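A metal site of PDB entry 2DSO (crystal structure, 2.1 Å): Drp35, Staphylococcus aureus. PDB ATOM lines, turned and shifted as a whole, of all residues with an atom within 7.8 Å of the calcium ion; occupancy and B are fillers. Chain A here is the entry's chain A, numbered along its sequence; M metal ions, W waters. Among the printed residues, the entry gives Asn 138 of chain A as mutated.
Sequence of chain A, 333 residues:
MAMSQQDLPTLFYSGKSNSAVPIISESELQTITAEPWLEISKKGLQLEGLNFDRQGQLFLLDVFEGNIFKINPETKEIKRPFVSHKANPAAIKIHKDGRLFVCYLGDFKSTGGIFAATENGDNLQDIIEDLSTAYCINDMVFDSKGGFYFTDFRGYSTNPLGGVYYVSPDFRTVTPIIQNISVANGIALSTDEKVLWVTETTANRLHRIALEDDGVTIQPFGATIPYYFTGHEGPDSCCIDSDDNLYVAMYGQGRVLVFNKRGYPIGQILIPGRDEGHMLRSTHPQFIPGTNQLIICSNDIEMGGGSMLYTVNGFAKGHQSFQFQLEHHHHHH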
ATOM      1  N   LEU A  47      25.442 -18.580  24.102  1.00  0.00           N
ATOM      2  CA  LEU A  47      25.210 -17.928  22.814  1.00  0.00           C
ATOM      3  C   LEU A  47      24.924 -16.433  22.931  1.00  0.00           C
ATOM      4  O   LEU A  47      24.228 -15.982  23.847  1.00  0.00           O
ATOM      5  CB  LEU A  47      24.047 -18.606  22.073  1.00  0.00           C
ATOM      6  CG  LEU A  47      24.175 -20.108  21.779  1.00  0.00           C
ATOM      7  CD1 LEU A  47      22.994 -20.558  20.917  1.00  0.00           C
ATOM      8  CD2 LEU A  47      25.488 -20.373  21.054  1.00  0.00           C
ATOM      9  N   GLU A  48      25.468 -15.659  21.982  1.00  0.00           N
ATOM     10  CA  GLU A  48      25.295 -14.212  21.950  1.00  0.00           C
ATOM     11  C   GLU A  48      25.744 -13.645  20.609  1.00  0.00           C
ATOM     12  O   GLU A  48      26.243 -14.376  19.748  1.00  0.00           O
ATOM     13  CB  GLU A  48      26.122 -13.565  23.063  1.00  0.00           C
ATOM     14  CG  GLU A  48      25.312 -12.983  24.206  1.00  0.00           C
ATOM     15  CD  GLU A  48      24.742 -11.610  23.888  1.00  0.00           C
ATOM     16  OE1 GLU A  48      24.215 -11.423  22.772  1.00  0.00           O
ATOM     17  OE2 GLU A  48      24.810 -10.713  24.761  1.00  0.00           O
ATOM     18  N   GLY A  49      25.545 -12.342  20.432  1.00  0.00           N
ATOM     19  CA  GLY A  49      25.968 -11.641  19.239  1.00  0.00           C
ATOM     20  C   GLY A  49      25.425 -11.993  17.857  1.00  0.00           C
ATOM     21  O   GLY A  49      26.195 -12.057  16.902  1.00  0.00           O
ATOM     22  N   ALA A  90      31.311 -10.863  23.315  1.00  0.00           N
ATOM     23  CA  ALA A  90      29.876 -10.815  23.626  1.00  0.00           C
ATOM     24  C   ALA A  90      28.970 -10.344  22.496  1.00  0.00           C
ATOM     25  O   ALA A  90      27.745 -10.514  22.567  1.00  0.00           O
ATOM     26  CB  ALA A  90      29.657  -9.932  24.854  1.00  0.00           C
ATOM     27  N   ALA A  91      29.540  -9.762  21.459  1.00  0.00           N
ATOM     28  CA  ALA A  91      28.733  -9.294  20.346  1.00  0.00           C
ATOM     29  C   ALA A  91      29.495  -9.198  19.036  1.00  0.00           C
ATOM     30  O   ALA A  91      30.713  -8.969  19.017  1.00  0.00           O
ATOM     31  CB  ALA A  91      28.104  -7.949  20.679  1.00  0.00           C
ATOM     32  N   LYS A  93      29.060  -7.240  15.265  1.00  0.00           N
ATOM     33  CA  LYS A  93      28.378  -6.269  14.419  1.00  0.00           C
ATOM     34  C   LYS A  93      29.192  -6.179  13.139  1.00  0.00           C
ATOM     35  O   LYS A  93      30.379  -5.838  13.159  1.00  0.00           O
ATOM     36  CB  LYS A  93      28.320  -4.894  15.083  1.00  0.00           C
ATOM     37  CG  LYS A  93      26.933  -4.506  15.572  1.00  0.00           C
ATOM     38  CD  LYS A  93      26.408  -5.488  16.619  1.00  0.00           C
ATOM     39  CE  LYS A  93      24.950  -5.215  16.951  1.00  0.00           C
ATOM     40  NZ  LYS A  93      24.479  -6.089  18.082  1.00  0.00           N
ATOM     41  N   LEU A 105      34.386  -8.713  26.705  1.00  0.00           N
ATOM     42  CA  LEU A 105      34.414  -8.267  28.083  1.00  0.00           C
ATOM     43  C   LEU A 105      35.758  -8.463  28.797  1.00  0.00           C
ATOM     44  O   LEU A 105      36.011  -7.845  29.824  1.00  0.00           O
ATOM     45  CB  LEU A 105      33.298  -8.993  28.853  1.00  0.00           C
ATOM     46  CG  LEU A 105      31.936  -8.861  28.178  1.00  0.00           C
ATOM     47  CD1 LEU A 105      30.936  -9.799  28.836  1.00  0.00           C
ATOM     48  CD2 LEU A 105      31.461  -7.406  28.251  1.00  0.00           C
ATOM     49  N   ASN A 138      30.153  -4.820  25.770  1.00  0.00           N
ATOM     50  CA  ASN A 138      29.189  -5.873  25.530  1.00  0.00           C
ATOM     51  C   ASN A 138      28.507  -5.833  24.166  1.00  0.00           C
ATOM     52  O   ASN A 138      28.251  -6.882  23.575  1.00  0.00           O
ATOM     53  CB  ASN A 138      28.108  -5.846  26.626  1.00  0.00           C
ATOM     54  CG  ASN A 138      27.184  -7.037  26.558  1.00  0.00           C
ATOM     55  OD1 ASN A 138      26.314  -7.129  25.688  1.00  0.00           O
ATOM     56  ND2 ASN A 138      27.361  -7.971  27.482  1.00  0.00           N
ATOM     57  N   ASP A 139      28.226  -4.636  23.655  1.00  0.00           N
ATOM     58  CA  ASP A 139      27.551  -4.523  22.363  1.00  0.00           C
ATOM     59  C   ASP A 139      27.854  -3.176  21.715  1.00  0.00           C
ATOM     60  O   ASP A 139      28.483  -2.315  22.322  1.00  0.00           O
ATOM     61  CB  ASP A 139      26.039  -4.672  22.549  1.00  0.00           C
ATOM     62  CG  ASP A 139      25.358  -5.330  21.347  1.00  0.00           C
ATOM     63  OD1 ASP A 139      25.775  -5.080  20.195  1.00  0.00           O
ATOM     64  OD2 ASP A 139      24.389  -6.107  21.554  1.00  0.00           O
ATOM     65  N   THR A 151      28.414  -0.110  24.461  1.00  0.00           N
ATOM     66  CA  THR A 151      28.054  -0.178  25.870  1.00  0.00           C
ATOM     67  C   THR A 151      29.199  -0.678  26.744  1.00  0.00           C
ATOM     68  O   THR A 151      29.817  -1.710  26.452  1.00  0.00           O
ATOM     69  CB  THR A 151      26.830  -1.098  26.101  1.00  0.00           C
ATOM     70  OG1 THR A 151      27.057  -2.369  25.488  1.00  0.00           O
ATOM     71  CG2 THR A 151      25.583  -0.469  25.508  1.00  0.00           C
ATOM     72  N   PHE A 153      30.088  -2.414  29.773  1.00  0.00           N
ATOM     73  CA  PHE A 153      29.501  -3.436  30.642  1.00  0.00           C
ATOM     74  C   PHE A 153      30.285  -3.584  31.947  1.00  0.00           C
ATOM     75  O   PHE A 153      30.999  -4.575  32.124  1.00  0.00           O
ATOM     76  CB  PHE A 153      29.534  -4.768  29.876  1.00  0.00           C
ATOM     77  CG  PHE A 153      28.635  -5.828  30.425  1.00  0.00           C
ATOM     78  CD1 PHE A 153      27.267  -5.819  30.137  1.00  0.00           C
ATOM     79  CD2 PHE A 153      29.154  -6.907  31.140  1.00  0.00           C
ATOM     80  CE1 PHE A 153      26.447  -6.860  30.553  1.00  0.00           C
ATOM     81  CE2 PHE A 153      28.339  -7.956  31.558  1.00  0.00           C
ATOM     82  CZ  PHE A 153      26.984  -7.930  31.258  1.00  0.00           C
ATOM     83  N   ALA A 184      25.806  -1.203  31.306  1.00  0.00           N
ATOM     84  CA  ALA A 184      25.086  -0.957  30.067  1.00  0.00           C
ATOM     85  C   ALA A 184      25.266  -2.236  29.264  1.00  0.00           C
ATOM     86  O   ALA A 184      26.362  -2.795  29.207  1.00  0.00           O
ATOM     87  CB  ALA A 184      25.685   0.232  29.327  1.00  0.00           C
ATOM     88  N   ASN A 185      24.204  -2.716  28.641  1.00  0.00           N
ATOM     89  CA  ASN A 185      24.272  -3.959  27.886  1.00  0.00           C
ATOM     90  C   ASN A 185      23.782  -3.769  26.457  1.00  0.00           C
ATOM     91  O   ASN A 185      24.569  -3.577  25.535  1.00  0.00           O
ATOM     92  CB  ASN A 185      23.438  -5.018  28.599  1.00  0.00           C
ATOM     93  CG  ASN A 185      23.683  -6.427  28.073  1.00  0.00           C
ATOM     94  OD1 ASN A 185      23.883  -6.634  26.877  1.00  0.00           O
ATOM     95  ND2 ASN A 185      23.625  -7.405  28.967  1.00  0.00           N
ATOM     96  N   GLY A 186      22.460  -3.835  26.280  1.00  0.00           N
ATOM     97  CA  GLY A 186      21.884  -3.687  24.957  1.00  0.00           C
ATOM     98  C   GLY A 186      21.915  -2.254  24.447  1.00  0.00           C
ATOM     99  O   GLY A 186      21.891  -1.306  25.235  1.00  0.00           O
ATOM    100  N   ILE A 187      21.972  -2.107  23.131  1.00  0.00           N
ATOM    101  CA  ILE A 187      21.998  -0.786  22.536  1.00  0.00           C
ATOM    102  C   ILE A 187      21.456  -0.838  21.117  1.00  0.00           C
ATOM    103  O   ILE A 187      21.688  -1.792  20.383  1.00  0.00           O
ATOM    104  CB  ILE A 187      23.431  -0.199  22.524  1.00  0.00           C
ATOM    105  CG1 ILE A 187      23.397   1.283  22.130  1.00  0.00           C
ATOM    106  CG2 ILE A 187      24.324  -1.001  21.552  1.00  0.00           C
ATOM    107  CD1 ILE A 187      24.721   1.993  22.348  1.00  0.00           C
ATOM    108  N   THR A 199      19.899  -0.740  27.425  1.00  0.00           N
ATOM    109  CA  THR A 199      19.363  -1.517  28.530  1.00  0.00           C
ATOM    110  C   THR A 199      20.407  -1.590  29.638  1.00  0.00           C
ATOM    111  O   THR A 199      21.594  -1.791  29.385  1.00  0.00           O
ATOM    112  CB  THR A 199      18.957  -2.959  28.101  1.00  0.00           C
ATOM    113  OG1 THR A 199      20.116  -3.691  27.693  1.00  0.00           O
ATOM    114  CG2 THR A 199      17.958  -2.915  26.954  1.00  0.00           C
ATOM    115  N   THR A 201      21.246  -3.707  32.617  1.00  0.00           N
ATOM    116  CA  THR A 201      20.991  -5.029  33.186  1.00  0.00           C
ATOM    117  C   THR A 201      20.808  -5.185  34.699  1.00  0.00           C
ATOM    118  O   THR A 201      19.825  -5.782  35.152  1.00  0.00           O
ATOM    119  CB  THR A 201      22.074  -6.019  32.745  1.00  0.00           C
ATOM    120  OG1 THR A 201      22.169  -6.025  31.316  1.00  0.00           O
ATOM    121  CG2 THR A 201      21.725  -7.429  33.222  1.00  0.00           C
ATOM    122  N   PRO A 235      17.515  -6.881  31.613  1.00  0.00           N
ATOM    123  CA  PRO A 235      17.526  -6.728  30.156  1.00  0.00           C
ATOM    124  C   PRO A 235      18.914  -6.970  29.562  1.00  0.00           C
ATOM    125  O   PRO A 235      19.927  -6.593  30.163  1.00  0.00           O
ATOM    126  CB  PRO A 235      17.002  -5.290  29.968  1.00  0.00           C
ATOM    127  CG  PRO A 235      17.487  -4.597  31.195  1.00  0.00           C
ATOM    128  CD  PRO A 235      17.233  -5.606  32.288  1.00  0.00           C
ATOM    129  N   ASP A 236      18.943  -7.619  28.399  1.00  0.00           N
ATOM    130  CA  ASP A 236      20.195  -7.904  27.709  1.00  0.00           C
ATOM    131  C   ASP A 236      20.198  -7.200  26.347  1.00  0.00           C
ATOM    132  O   ASP A 236      19.820  -6.032  26.256  1.00  0.00           O
ATOM    133  CB  ASP A 236      20.371  -9.429  27.528  1.00  0.00           C
ATOM    134  CG  ASP A 236      21.845  -9.845  27.415  1.00  0.00           C
ATOM    135  OD1 ASP A 236      22.250 -10.778  28.130  1.00  0.00           O
ATOM    136  OD2 ASP A 236      22.594  -9.255  26.599  1.00  0.00           O
ATOM    137  N   SER A 237      20.591  -7.906  25.291  1.00  0.00           N
ATOM    138  CA  SER A 237      20.671  -7.300  23.968  1.00  0.00           C
ATOM    139  C   SER A 237      19.334  -6.959  23.314  1.00  0.00           C
ATOM    140  O   SER A 237      18.299  -7.542  23.624  1.00  0.00           O
ATOM    141  CB  SER A 237      21.468  -8.211  23.018  1.00  0.00           C
ATOM    142  OG  SER A 237      22.549  -8.817  23.705  1.00  0.00           O
ATOM    143  N   CYS A 238      19.379  -6.012  22.382  1.00  0.00           N
ATOM    144  CA  CYS A 238      18.180  -5.586  21.695  1.00  0.00           C
ATOM    145  C   CYS A 238      18.448  -5.207  20.243  1.00  0.00           C
ATOM    146  O   CYS A 238      19.590  -4.983  19.843  1.00  0.00           O
ATOM    147  CB  CYS A 238      17.561  -4.390  22.422  1.00  0.00           C
ATOM    148  SG  CYS A 238      18.682  -2.981  22.620  1.00  0.00           S
ATOM    149  N   ALA A 249      15.825  -8.855  24.642  1.00  0.00           N
ATOM    150  CA  ALA A 249      15.991 -10.188  25.208  1.00  0.00           C
ATOM    151  C   ALA A 249      16.177  -9.996  26.713  1.00  0.00           C
ATOM    152  O   ALA A 249      16.938  -9.138  27.158  1.00  0.00           O
ATOM    153  CB  ALA A 249      17.218 -10.881  24.589  1.00  0.00           C
ATOM    154  N   TYR A 251      17.661 -11.479  29.918  1.00  0.00           N
ATOM    155  CA  TYR A 251      18.588 -12.483  30.428  1.00  0.00           C
ATOM    156  C   TYR A 251      18.143 -13.159  31.726  1.00  0.00           C
ATOM    157  O   TYR A 251      17.917 -12.498  32.743  1.00  0.00           O
ATOM    158  CB  TYR A 251      19.976 -11.882  30.632  1.00  0.00           C
ATOM    159  CG  TYR A 251      21.023 -12.923  30.932  1.00  0.00           C
ATOM    160  CD1 TYR A 251      21.357 -13.887  29.990  1.00  0.00           C
ATOM    161  CD2 TYR A 251      21.671 -12.959  32.166  1.00  0.00           C
ATOM    162  CE1 TYR A 251      22.295 -14.873  30.263  1.00  0.00           C
ATOM    163  CE2 TYR A 251      22.620 -13.944  32.462  1.00  0.00           C
ATOM    164  CZ  TYR A 251      22.931 -14.891  31.503  1.00  0.00           C
ATOM    165  OH  TYR A 251      23.860 -15.864  31.752  1.00  0.00           O
ATOM    166  N   THR A 283      19.528 -14.215  25.328  1.00  0.00           N
ATOM    167  CA  THR A 283      20.433 -13.077  25.289  1.00  0.00           C
ATOM    168  C   THR A 283      20.402 -12.125  24.108  1.00  0.00           C
ATOM    169  O   THR A 283      20.812 -10.968  24.245  1.00  0.00           O
ATOM    170  CB  THR A 283      21.897 -13.563  25.402  1.00  0.00           C
ATOM    171  OG1 THR A 283      22.186 -14.416  24.292  1.00  0.00           O
ATOM    172  CG2 THR A 283      22.115 -14.336  26.686  1.00  0.00           C
ATOM    173  N   HIS A 284      19.926 -12.571  22.947  1.00  0.00           N
ATOM    174  CA  HIS A 284      19.963 -11.702  21.790  1.00  0.00           C
ATOM    175  C   HIS A 284      18.903 -11.999  20.728  1.00  0.00           C
ATOM    176  O   HIS A 284      18.652 -13.160  20.402  1.00  0.00           O
ATOM    177  CB  HIS A 284      21.362 -11.799  21.154  1.00  0.00           C
ATOM    178  CG  HIS A 284      21.821 -10.553  20.475  1.00  0.00           C
ATOM    179  ND1 HIS A 284      22.968  -9.880  20.865  1.00  0.00           N
ATOM    180  CD2 HIS A 284      21.295  -9.846  19.450  1.00  0.00           C
ATOM    181  CE1 HIS A 284      23.121  -8.817  20.095  1.00  0.00           C
ATOM    182  NE2 HIS A 284      22.122  -8.774  19.225  1.00  0.00           N
ATOM    183  N   PRO A 285      18.261 -10.946  20.183  1.00  0.00           N
ATOM    184  CA  PRO A 285      17.235 -11.100  19.155  1.00  0.00           C
ATOM    185  C   PRO A 285      17.746 -10.466  17.854  1.00  0.00           C
ATOM    186  O   PRO A 285      18.436  -9.443  17.891  1.00  0.00           O
ATOM    187  CB  PRO A 285      16.073 -10.322  19.740  1.00  0.00           C
ATOM    188  CG  PRO A 285      16.797  -9.100  20.254  1.00  0.00           C
ATOM    189  CD  PRO A 285      18.070  -9.662  20.892  1.00  0.00           C
HETATM  190 CA    CA M   1      24.300  -8.378  25.303  1.00  0.00          CA
HETATM  191  O   HOH W   1      23.925  -6.523  24.345  1.00  0.00           O
HETATM  192  O   HOH W   2      25.909  -8.585  23.386  1.00  0.00           O
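Water W1 bridges the side-chain carboxylate (OD2) of Asp 139 and the backbone carbonyl oxygen (O) of Asn 185.
Of the 26 residues printed, 5 come within 4 Å of the calcium ion.
Along chain A the residues within 4 Å of the calcium ion span positions 48 to 237.
The nearest printed residue that does not touch the calcium ion is Asp 139 (4.4 Å).
The calcium ion is bound by water W1 (2.1 Å), OD2 of Asp 236 (2.3 Å), OD1 of Asn 185 (2.4 Å), OD1 of Asn 138 (2.4 Å), OG of Ser 237 (2.4 Å), OE2 of Glu 48 (2.5 Å) and water W2 (2.5 Å).
The calcium ion has seven donor atoms within binding distance.
The backbone NH of Gly 186 lies close to the backbone carbonyl oxygen of Asp 236 (3.4 Å).
The backbone carbonyl oxygen (O) of Asn 185 sits at hydrogen-bond distance from the side-chain hydroxyl (OG1) of Thr 151.
The backbone NH (N) of Asn 185 is in hydrogen-bond range of the backbone carbonyl oxygen (O) of Thr 199 (2.9 Å).
ND2 of Asn 185 sits at hydrogen-bond distance from OG1 of Thr 201 (3.1 Å).
The backbone NH (N) of Asn 138 is in hydrogen-bond range of the backbone carbonyl oxygen (O) of Thr 151 (3.2 Å).
N of Ser 237 lies close to O of Thr 283, 3.2 Å away.
OG of Ser 237 lies close to ND1 of His 284 (3.1 Å).
N of Ala 249 sits at hydrogen-bond distance from O of Ser 237, at 3.0 Å.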
